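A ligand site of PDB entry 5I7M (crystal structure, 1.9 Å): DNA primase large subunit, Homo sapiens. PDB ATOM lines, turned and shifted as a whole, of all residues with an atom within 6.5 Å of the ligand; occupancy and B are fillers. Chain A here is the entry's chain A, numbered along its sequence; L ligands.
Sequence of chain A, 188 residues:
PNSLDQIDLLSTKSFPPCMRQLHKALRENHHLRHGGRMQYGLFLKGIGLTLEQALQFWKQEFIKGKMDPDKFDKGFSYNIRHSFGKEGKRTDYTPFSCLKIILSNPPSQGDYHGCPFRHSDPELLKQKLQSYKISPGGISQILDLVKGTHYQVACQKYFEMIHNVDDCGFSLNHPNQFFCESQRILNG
The backbone carbonyl oxygen (O) of Asn 173 lies within hydrogen-bond range of the backbone NH (N) of Cys 98, at 3.2 Å. The side-chain sulfur (SG) of Cys 98 lies close to the backbone NH (N) of His 174 (3.3 Å). The backbone NH of Phe 117 sits close to the side-chain sulfur of Cys 115, at 3.7 Å.
CB of Pro 16 touches S2 of the ligand, 3.7 Å away. CE2 of Phe 117 touches S4 of the ligand (3.95 Å). Hydrophobic or aromatic side chains within 4 Å of the ligand: Pro 16 and Phe 117. Of the 25 residues printed, 6 come within 4 Å of the ligand.
An iron atom (FE4) of the ligand is bound by the side-chain sulfur (SG) of Cys 98. The side-chain sulfur of Cys 115 binds an iron atom (FE2) of the ligand (2.2 Å). The side-chain sulfur of Cys 18 binds an iron atom (FE3) of the ligand (2.1 Å). A sulfur (S4) of the ligand sits close to the backbone NH (N) of Cys 18 (3.7 Å). The side-chain sulfur (SG) of Cys 155 is bound to an iron atom (FE1) of the ligand (2.1 Å).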
ATOM      1  N   PRO A  16      17.628  22.076  -6.544  1.00  0.00           N
ATOM      2  CA  PRO A  16      19.059  22.173  -6.248  1.00  0.00           C
ATOM      3  C   PRO A  16      19.465  23.653  -6.284  1.00  0.00           C
ATOM      4  O   PRO A  16      18.739  24.443  -6.887  1.00  0.00           O
ATOM      5  CB  PRO A  16      19.712  21.413  -7.396  1.00  0.00           C
ATOM      6  CG  PRO A  16      18.756  21.555  -8.524  1.00  0.00           C
ATOM      7  CD  PRO A  16      17.381  21.552  -7.906  1.00  0.00           C
ATOM      8  N   PRO A  17      20.582  24.003  -5.653  1.00  0.00           N
ATOM      9  CA  PRO A  17      21.045  25.396  -5.623  1.00  0.00           C
ATOM     10  C   PRO A  17      21.017  26.117  -6.972  1.00  0.00           C
ATOM     11  O   PRO A  17      20.667  27.294  -7.028  1.00  0.00           O
ATOM     12  CB  PRO A  17      22.493  25.269  -5.128  1.00  0.00           C
ATOM     13  CG  PRO A  17      22.500  24.021  -4.318  1.00  0.00           C
ATOM     14  CD  PRO A  17      21.520  23.092  -4.994  1.00  0.00           C
ATOM     15  N   CYS A  18      21.389  25.413  -8.046  1.00  0.00           N
ATOM     16  CA  CYS A  18      21.420  25.988  -9.360  1.00  0.00           C
ATOM     17  C   CYS A  18      20.020  26.371  -9.928  1.00  0.00           C
ATOM     18  O   CYS A  18      19.921  27.279 -10.736  1.00  0.00           O
ATOM     19  CB  CYS A  18      22.055  25.009 -10.323  1.00  0.00           C
ATOM     20  SG  CYS A  18      21.184  23.410 -10.513  1.00  0.00           S
ATOM     21  N   MET A  19      18.951  25.645  -9.542  1.00  0.00           N
ATOM     22  CA  MET A  19      17.630  25.984 -10.025  1.00  0.00           C
ATOM     23  C   MET A  19      16.949  26.895  -9.023  1.00  0.00           C
ATOM     24  O   MET A  19      16.129  27.747  -9.369  1.00  0.00           O
ATOM     25  CB  MET A  19      16.836  24.692 -10.255  1.00  0.00           C
ATOM     26  CG  MET A  19      17.462  23.732 -11.224  1.00  0.00           C
ATOM     27  SD  MET A  19      17.822  24.382 -12.838  1.00  0.00           S
ATOM     28  CE  MET A  19      18.666  22.956 -13.560  1.00  0.00           C
ATOM     29  N   GLN A  39      18.240  26.706 -18.899  1.00  0.00           N
ATOM     30  CA  GLN A  39      18.584  25.844 -17.786  1.00  0.00           C
ATOM     31  C   GLN A  39      17.375  25.623 -16.904  1.00  0.00           C
ATOM     32  O   GLN A  39      17.039  24.445 -16.640  1.00  0.00           O
ATOM     33  CB  GLN A  39      19.747  26.390 -16.949  1.00  0.00           C
ATOM     34  CG  GLN A  39      20.165  25.507 -15.821  1.00  0.00           C
ATOM     35  CD  GLN A  39      21.461  25.958 -15.204  1.00  0.00           C
ATOM     36  OE1 GLN A  39      22.406  26.350 -15.910  1.00  0.00           O
ATOM     37  NE2 GLN A  39      21.517  25.903 -13.908  1.00  0.00           N
ATOM     38  N   SER A  97      22.219  18.095 -17.596  1.00  0.00           N
ATOM     39  CA  SER A  97      22.869  17.362 -16.480  1.00  0.00           C
ATOM     40  C   SER A  97      23.836  18.294 -15.682  1.00  0.00           C
ATOM     41  O   SER A  97      24.189  19.413 -16.148  1.00  0.00           O
ATOM     42  CB  SER A  97      23.726  16.233 -17.022  1.00  0.00           C
ATOM     43  OG  SER A  97      24.865  16.854 -17.610  1.00  0.00           O
ATOM     44  N   CYS A  98      24.311  17.803 -14.532  1.00  0.00           N
ATOM     45  CA  CYS A  98      25.231  18.571 -13.717  1.00  0.00           C
ATOM     46  C   CYS A  98      26.525  18.863 -14.503  1.00  0.00           C
ATOM     47  O   CYS A  98      26.967  20.001 -14.482  1.00  0.00           O
ATOM     48  CB  CYS A  98      25.614  17.835 -12.433  1.00  0.00           C
ATOM     49  SG  CYS A  98      24.339  17.710 -11.167  1.00  0.00           S
ATOM     50  N   LEU A  99      27.075  17.879 -15.204  1.00  0.00           N
ATOM     51  CA  LEU A  99      28.312  18.105 -15.959  1.00  0.00           C
ATOM     52  C   LEU A  99      28.153  19.138 -17.052  1.00  0.00           C
ATOM     53  O   LEU A  99      29.062  19.973 -17.249  1.00  0.00           O
ATOM     54  CB  LEU A  99      28.862  16.814 -16.580  1.00  0.00           C
ATOM     55  CG  LEU A  99      29.506  15.809 -15.590  1.00  0.00           C
ATOM     56  CD1 LEU A  99      30.204  14.674 -16.359  1.00  0.00           C
ATOM     57  CD2 LEU A  99      30.445  16.479 -14.592  1.00  0.00           C
ATOM     58  N   ILE A 101      26.046  21.725 -17.004  1.00  0.00           N
ATOM     59  CA  ILE A 101      25.925  22.980 -16.302  1.00  0.00           C
ATOM     60  C   ILE A 101      27.291  23.451 -15.794  1.00  0.00           C
ATOM     61  O   ILE A 101      27.633  24.577 -15.964  1.00  0.00           O
ATOM     62  CB  ILE A 101      24.925  22.855 -15.147  1.00  0.00           C
ATOM     63  CG1 ILE A 101      23.524  22.573 -15.709  1.00  0.00           C
ATOM     64  CG2 ILE A 101      24.973  24.081 -14.251  1.00  0.00           C
ATOM     65  CD1 ILE A 101      22.509  22.103 -14.700  1.00  0.00           C
ATOM     66  N   ILE A 102      28.037  22.562 -15.176  1.00  0.00           N
ATOM     67  CA  ILE A 102      29.338  22.864 -14.618  1.00  0.00           C
ATOM     68  C   ILE A 102      30.429  23.176 -15.664  1.00  0.00           C
ATOM     69  O   ILE A 102      31.191  24.104 -15.527  1.00  0.00           O
ATOM     70  CB  ILE A 102      29.797  21.734 -13.670  1.00  0.00           C
ATOM     71  CG1 ILE A 102      28.927  21.685 -12.440  1.00  0.00           C
ATOM     72  CG2 ILE A 102      31.244  21.882 -13.239  1.00  0.00           C
ATOM     73  CD1 ILE A 102      29.145  20.485 -11.596  1.00  0.00           C
ATOM     74  N   GLY A 114      24.173  28.369 -14.488  1.00  0.00           N
ATOM     75  CA  GLY A 114      25.360  27.688 -13.971  1.00  0.00           C
ATOM     76  C   GLY A 114      25.124  26.934 -12.689  1.00  0.00           C
ATOM     77  O   GLY A 114      23.973  26.729 -12.287  1.00  0.00           O
ATOM     78  N   CYS A 115      26.221  26.473 -12.077  1.00  0.00           N
ATOM     79  CA  CYS A 115      26.272  25.793 -10.805  1.00  0.00           C
ATOM     80  C   CYS A 115      26.948  26.633  -9.725  1.00  0.00           C
ATOM     81  O   CYS A 115      28.130  26.925  -9.897  1.00  0.00           O
ATOM     82  CB  CYS A 115      27.046  24.478 -11.019  1.00  0.00           C
ATOM     83  SG  CYS A 115      27.322  23.635  -9.450  1.00  0.00           S
ATOM     84  N   PRO A 116      26.248  27.029  -8.628  1.00  0.00           N
ATOM     85  CA  PRO A 116      26.816  27.987  -7.668  1.00  0.00           C
ATOM     86  C   PRO A 116      28.070  27.403  -6.966  1.00  0.00           C
ATOM     87  O   PRO A 116      28.949  28.164  -6.557  1.00  0.00           O
ATOM     88  CB  PRO A 116      25.754  28.172  -6.617  1.00  0.00           C
ATOM     89  CG  PRO A 116      24.498  27.598  -7.248  1.00  0.00           C
ATOM     90  CD  PRO A 116      24.913  26.591  -8.227  1.00  0.00           C
ATOM     91  N   PHE A 117      28.146  26.073  -6.854  1.00  0.00           N
ATOM     92  CA  PHE A 117      29.381  25.464  -6.333  1.00  0.00           C
ATOM     93  C   PHE A 117      30.615  25.684  -7.227  1.00  0.00           C
ATOM     94  O   PHE A 117      31.684  25.821  -6.696  1.00  0.00           O
ATOM     95  CB  PHE A 117      29.193  23.951  -6.037  1.00  0.00           C
ATOM     96  CG  PHE A 117      28.070  23.692  -5.112  1.00  0.00           C
ATOM     97  CD1 PHE A 117      28.147  24.125  -3.790  1.00  0.00           C
ATOM     98  CD2 PHE A 117      26.860  23.158  -5.592  1.00  0.00           C
ATOM     99  CE1 PHE A 117      27.068  23.948  -2.946  1.00  0.00           C
ATOM    100  CE2 PHE A 117      25.808  22.951  -4.755  1.00  0.00           C
ATOM    101  CZ  PHE A 117      25.908  23.334  -3.395  1.00  0.00           C
ATOM    102  N   ARG A 118      30.432  25.652  -8.535  1.00  0.00           N
ATOM    103  CA  ARG A 118      31.473  25.829  -9.530  1.00  0.00           C
ATOM    104  C   ARG A 118      31.670  27.291  -9.876  1.00  0.00           C
ATOM    105  O   ARG A 118      32.809  27.748 -10.064  1.00  0.00           O
ATOM    106  CB  ARG A 118      31.127  25.081 -10.813  1.00  0.00           C
ATOM    107  CG  ARG A 118      31.851  25.482 -12.109  1.00  0.00           C
ATOM    108  CD  ARG A 118      33.310  25.113 -12.152  1.00  0.00           C
ATOM    109  NE  ARG A 118      33.873  25.573 -13.412  1.00  0.00           N
ATOM    110  CZ  ARG A 118      34.251  26.849 -13.645  1.00  0.00           C
ATOM    111  NH1 ARG A 118      34.117  27.784 -12.686  1.00  0.00           N
ATOM    112  NH2 ARG A 118      34.692  27.196 -14.848  1.00  0.00           N
ATOM    113  N   TYR A 151      32.172  19.603  -6.714  1.00  0.00           N
ATOM    114  CA  TYR A 151      30.963  20.341  -6.775  1.00  0.00           C
ATOM    115  C   TYR A 151      29.713  19.509  -6.477  1.00  0.00           C
ATOM    116  O   TYR A 151      28.902  19.907  -5.715  1.00  0.00           O
ATOM    117  CB  TYR A 151      30.896  21.047  -8.125  1.00  0.00           C
ATOM    118  CG  TYR A 151      32.155  21.797  -8.494  1.00  0.00           C
ATOM    119  CD1 TYR A 151      32.649  22.775  -7.680  1.00  0.00           C
ATOM    120  CD2 TYR A 151      32.827  21.553  -9.642  1.00  0.00           C
ATOM    121  CE1 TYR A 151      33.799  23.459  -7.996  1.00  0.00           C
ATOM    122  CE2 TYR A 151      33.970  22.229  -9.975  1.00  0.00           C
ATOM    123  CZ  TYR A 151      34.442  23.181  -9.140  1.00  0.00           C
ATOM    124  OH  TYR A 151      35.567  23.883  -9.442  1.00  0.00           O
ATOM    125  N   GLN A 152      29.611  18.361  -7.093  1.00  0.00           N
ATOM    126  CA  GLN A 152      28.462  17.490  -6.924  1.00  0.00           C
ATOM    127  C   GLN A 152      28.372  16.894  -5.528  1.00  0.00           C
ATOM    128  O   GLN A 152      27.330  16.756  -4.991  1.00  0.00           O
ATOM    129  CB  GLN A 152      28.462  16.457  -8.006  1.00  0.00           C
ATOM    130  CG  GLN A 152      28.267  17.105  -9.334  1.00  0.00           C
ATOM    131  CD  GLN A 152      28.754  16.335 -10.517  1.00  0.00           C
ATOM    132  OE1 GLN A 152      29.659  16.727 -11.171  1.00  0.00           O
ATOM    133  NE2 GLN A 152      28.126  15.238 -10.792  1.00  0.00           N
ATOM    134  N   VAL A 153      29.503  16.596  -4.928  1.00  0.00           N
ATOM    135  CA  VAL A 153      29.513  16.054  -3.552  1.00  0.00           C
ATOM    136  C   VAL A 153      29.178  17.186  -2.621  1.00  0.00           C
ATOM    137  O   VAL A 153      28.501  17.005  -1.629  1.00  0.00           O
ATOM    138  CB  VAL A 153      30.884  15.387  -3.165  1.00  0.00           C
ATOM    139  CG1 VAL A 153      30.876  14.841  -1.756  1.00  0.00           C
ATOM    140  CG2 VAL A 153      31.233  14.303  -4.138  1.00  0.00           C
ATOM    141  N   CYS A 155      27.097  19.468  -3.357  1.00  0.00           N
ATOM    142  CA  CYS A 155      25.625  19.587  -3.530  1.00  0.00           C
ATOM    143  C   CYS A 155      24.861  18.453  -2.759  1.00  0.00           C
ATOM    144  O   CYS A 155      23.749  18.665  -2.211  1.00  0.00           O
ATOM    145  CB  CYS A 155      25.302  19.543  -5.013  1.00  0.00           C
ATOM    146  SG  CYS A 155      23.609  20.062  -5.422  1.00  0.00           S
ATOM    147  N   GLN A 156      25.460  17.258  -2.713  1.00  0.00           N
ATOM    148  CA  GLN A 156      24.868  16.142  -1.855  1.00  0.00           C
ATOM    149  C   GLN A 156      24.895  16.501  -0.430  1.00  0.00           C
ATOM    150  O   GLN A 156      23.955  16.255   0.345  1.00  0.00           O
ATOM    151  CB  GLN A 156      25.619  14.829  -2.072  1.00  0.00           C
ATOM    152  CG  GLN A 156      25.603  14.329  -3.504  1.00  0.00           C
ATOM    153  CD  GLN A 156      26.465  13.116  -3.769  1.00  0.00           C
ATOM    154  OE1 GLN A 156      26.512  12.616  -4.894  1.00  0.00           O
ATOM    155  NE2 GLN A 156      27.210  12.677  -2.765  1.00  0.00           N
ATOM    156  N   LEU A 172      24.815  11.873  -7.017  1.00  0.00           N
ATOM    157  CA  LEU A 172      24.271  12.983  -7.779  1.00  0.00           C
ATOM    158  C   LEU A 172      24.916  13.276  -9.097  1.00  0.00           C
ATOM    159  O   LEU A 172      26.099  13.478  -9.154  1.00  0.00           O
ATOM    160  CB  LEU A 172      24.379  14.233  -6.943  1.00  0.00           C
ATOM    161  CG  LEU A 172      23.919  15.520  -7.612  1.00  0.00           C
ATOM    162  CD1 LEU A 172      22.506  15.425  -8.131  1.00  0.00           C
ATOM    163  CD2 LEU A 172      24.056  16.651  -6.646  1.00  0.00           C
ATOM    164  N   ASN A 173      24.130  13.341 -10.162  1.00  0.00           N
ATOM    165  CA  ASN A 173      24.615  13.679 -11.460  1.00  0.00           C
ATOM    166  C   ASN A 173      23.666  14.527 -12.297  1.00  0.00           C
ATOM    167  O   ASN A 173      23.923  14.784 -13.404  1.00  0.00           O
ATOM    168  CB  ASN A 173      24.987  12.468 -12.262  1.00  0.00           C
ATOM    169  CG  ASN A 173      23.816  11.536 -12.468  1.00  0.00           C
ATOM    170  OD1 ASN A 173      22.852  11.908 -13.030  1.00  0.00           O
ATOM    171  ND2 ASN A 173      23.933  10.338 -11.987  1.00  0.00           N
ATOM    172  N   HIS A 174      22.555  14.942 -11.730  1.00  0.00           N
ATOM    173  CA  HIS A 174      21.521  15.659 -12.551  1.00  0.00           C
ATOM    174  C   HIS A 174      20.607  16.435 -11.613  1.00  0.00           C
ATOM    175  O   HIS A 174      20.116  15.902 -10.571  1.00  0.00           O
ATOM    176  CB  HIS A 174      20.718  14.658 -13.394  1.00  0.00           C
ATOM    177  CG  HIS A 174      20.067  15.235 -14.622  1.00  0.00           C
ATOM    178  ND1 HIS A 174      19.071  16.163 -14.554  1.00  0.00           N
ATOM    179  CD2 HIS A 174      20.310  15.040 -15.928  1.00  0.00           C
ATOM    180  CE1 HIS A 174      18.671  16.480 -15.780  1.00  0.00           C
ATOM    181  NE2 HIS A 174      19.452  15.858 -16.633  1.00  0.00           N
ATOM    182  N   PRO A 175      20.409  17.726 -11.916  1.00  0.00           N
ATOM    183  CA  PRO A 175      19.461  18.490 -11.101  1.00  0.00           C
ATOM    184  C   PRO A 175      18.047  17.800 -11.007  1.00  0.00           C
ATOM    185  O   PRO A 175      17.410  17.853  -9.957  1.00  0.00           O
ATOM    186  CB  PRO A 175      19.380  19.819 -11.873  1.00  0.00           C
ATOM    187  CG  PRO A 175      20.652  19.932 -12.634  1.00  0.00           C
ATOM    188  CD  PRO A 175      20.975  18.531 -13.003  1.00  0.00           C
ATOM    189  N   PHE A 178      18.084  15.148  -8.299  1.00  0.00           N
ATOM    190  CA  PHE A 178      18.051  15.805  -7.008  1.00  0.00           C
ATOM    191  C   PHE A 178      16.603  16.038  -6.594  1.00  0.00           C
ATOM    192  O   PHE A 178      16.194  15.694  -5.560  1.00  0.00           O
ATOM    193  CB  PHE A 178      18.817  17.106  -7.150  1.00  0.00           C
ATOM    194  CG  PHE A 178      18.927  17.884  -5.905  1.00  0.00           C
ATOM    195  CD1 PHE A 178      17.834  18.444  -5.334  1.00  0.00           C
ATOM    196  CD2 PHE A 178      20.159  18.106  -5.328  1.00  0.00           C
ATOM    197  CE1 PHE A 178      17.938  19.183  -4.197  1.00  0.00           C
ATOM    198  CE2 PHE A 178      20.269  18.822  -4.195  1.00  0.00           C
ATOM    199  CZ  PHE A 178      19.169  19.358  -3.621  1.00  0.00           C
HETATM  200 FE1  LIG L   1      23.819  20.669  -7.465  1.00  0.00          FE
HETATM  201 FE2  LIG L   1      25.675  22.209  -9.280  1.00  0.00          FE
HETATM  202 FE3  LIG L   1      22.718  22.089  -9.883  1.00  0.00          FE
HETATM  203 FE4  LIG L   1      24.433  19.624 -10.224  1.00  0.00          FE
HETATM  204  S1  LIG L   1      24.506  21.630 -10.963  1.00  0.00           S
HETATM  205  S2  LIG L   1      22.650  20.090  -9.148  1.00  0.00           S
HETATM  206  S3  LIG L   1      25.602  20.203  -8.540  1.00  0.00           S
HETATM  207  S4  LIG L   1      23.894  22.661  -8.199  1.00  0.00           S
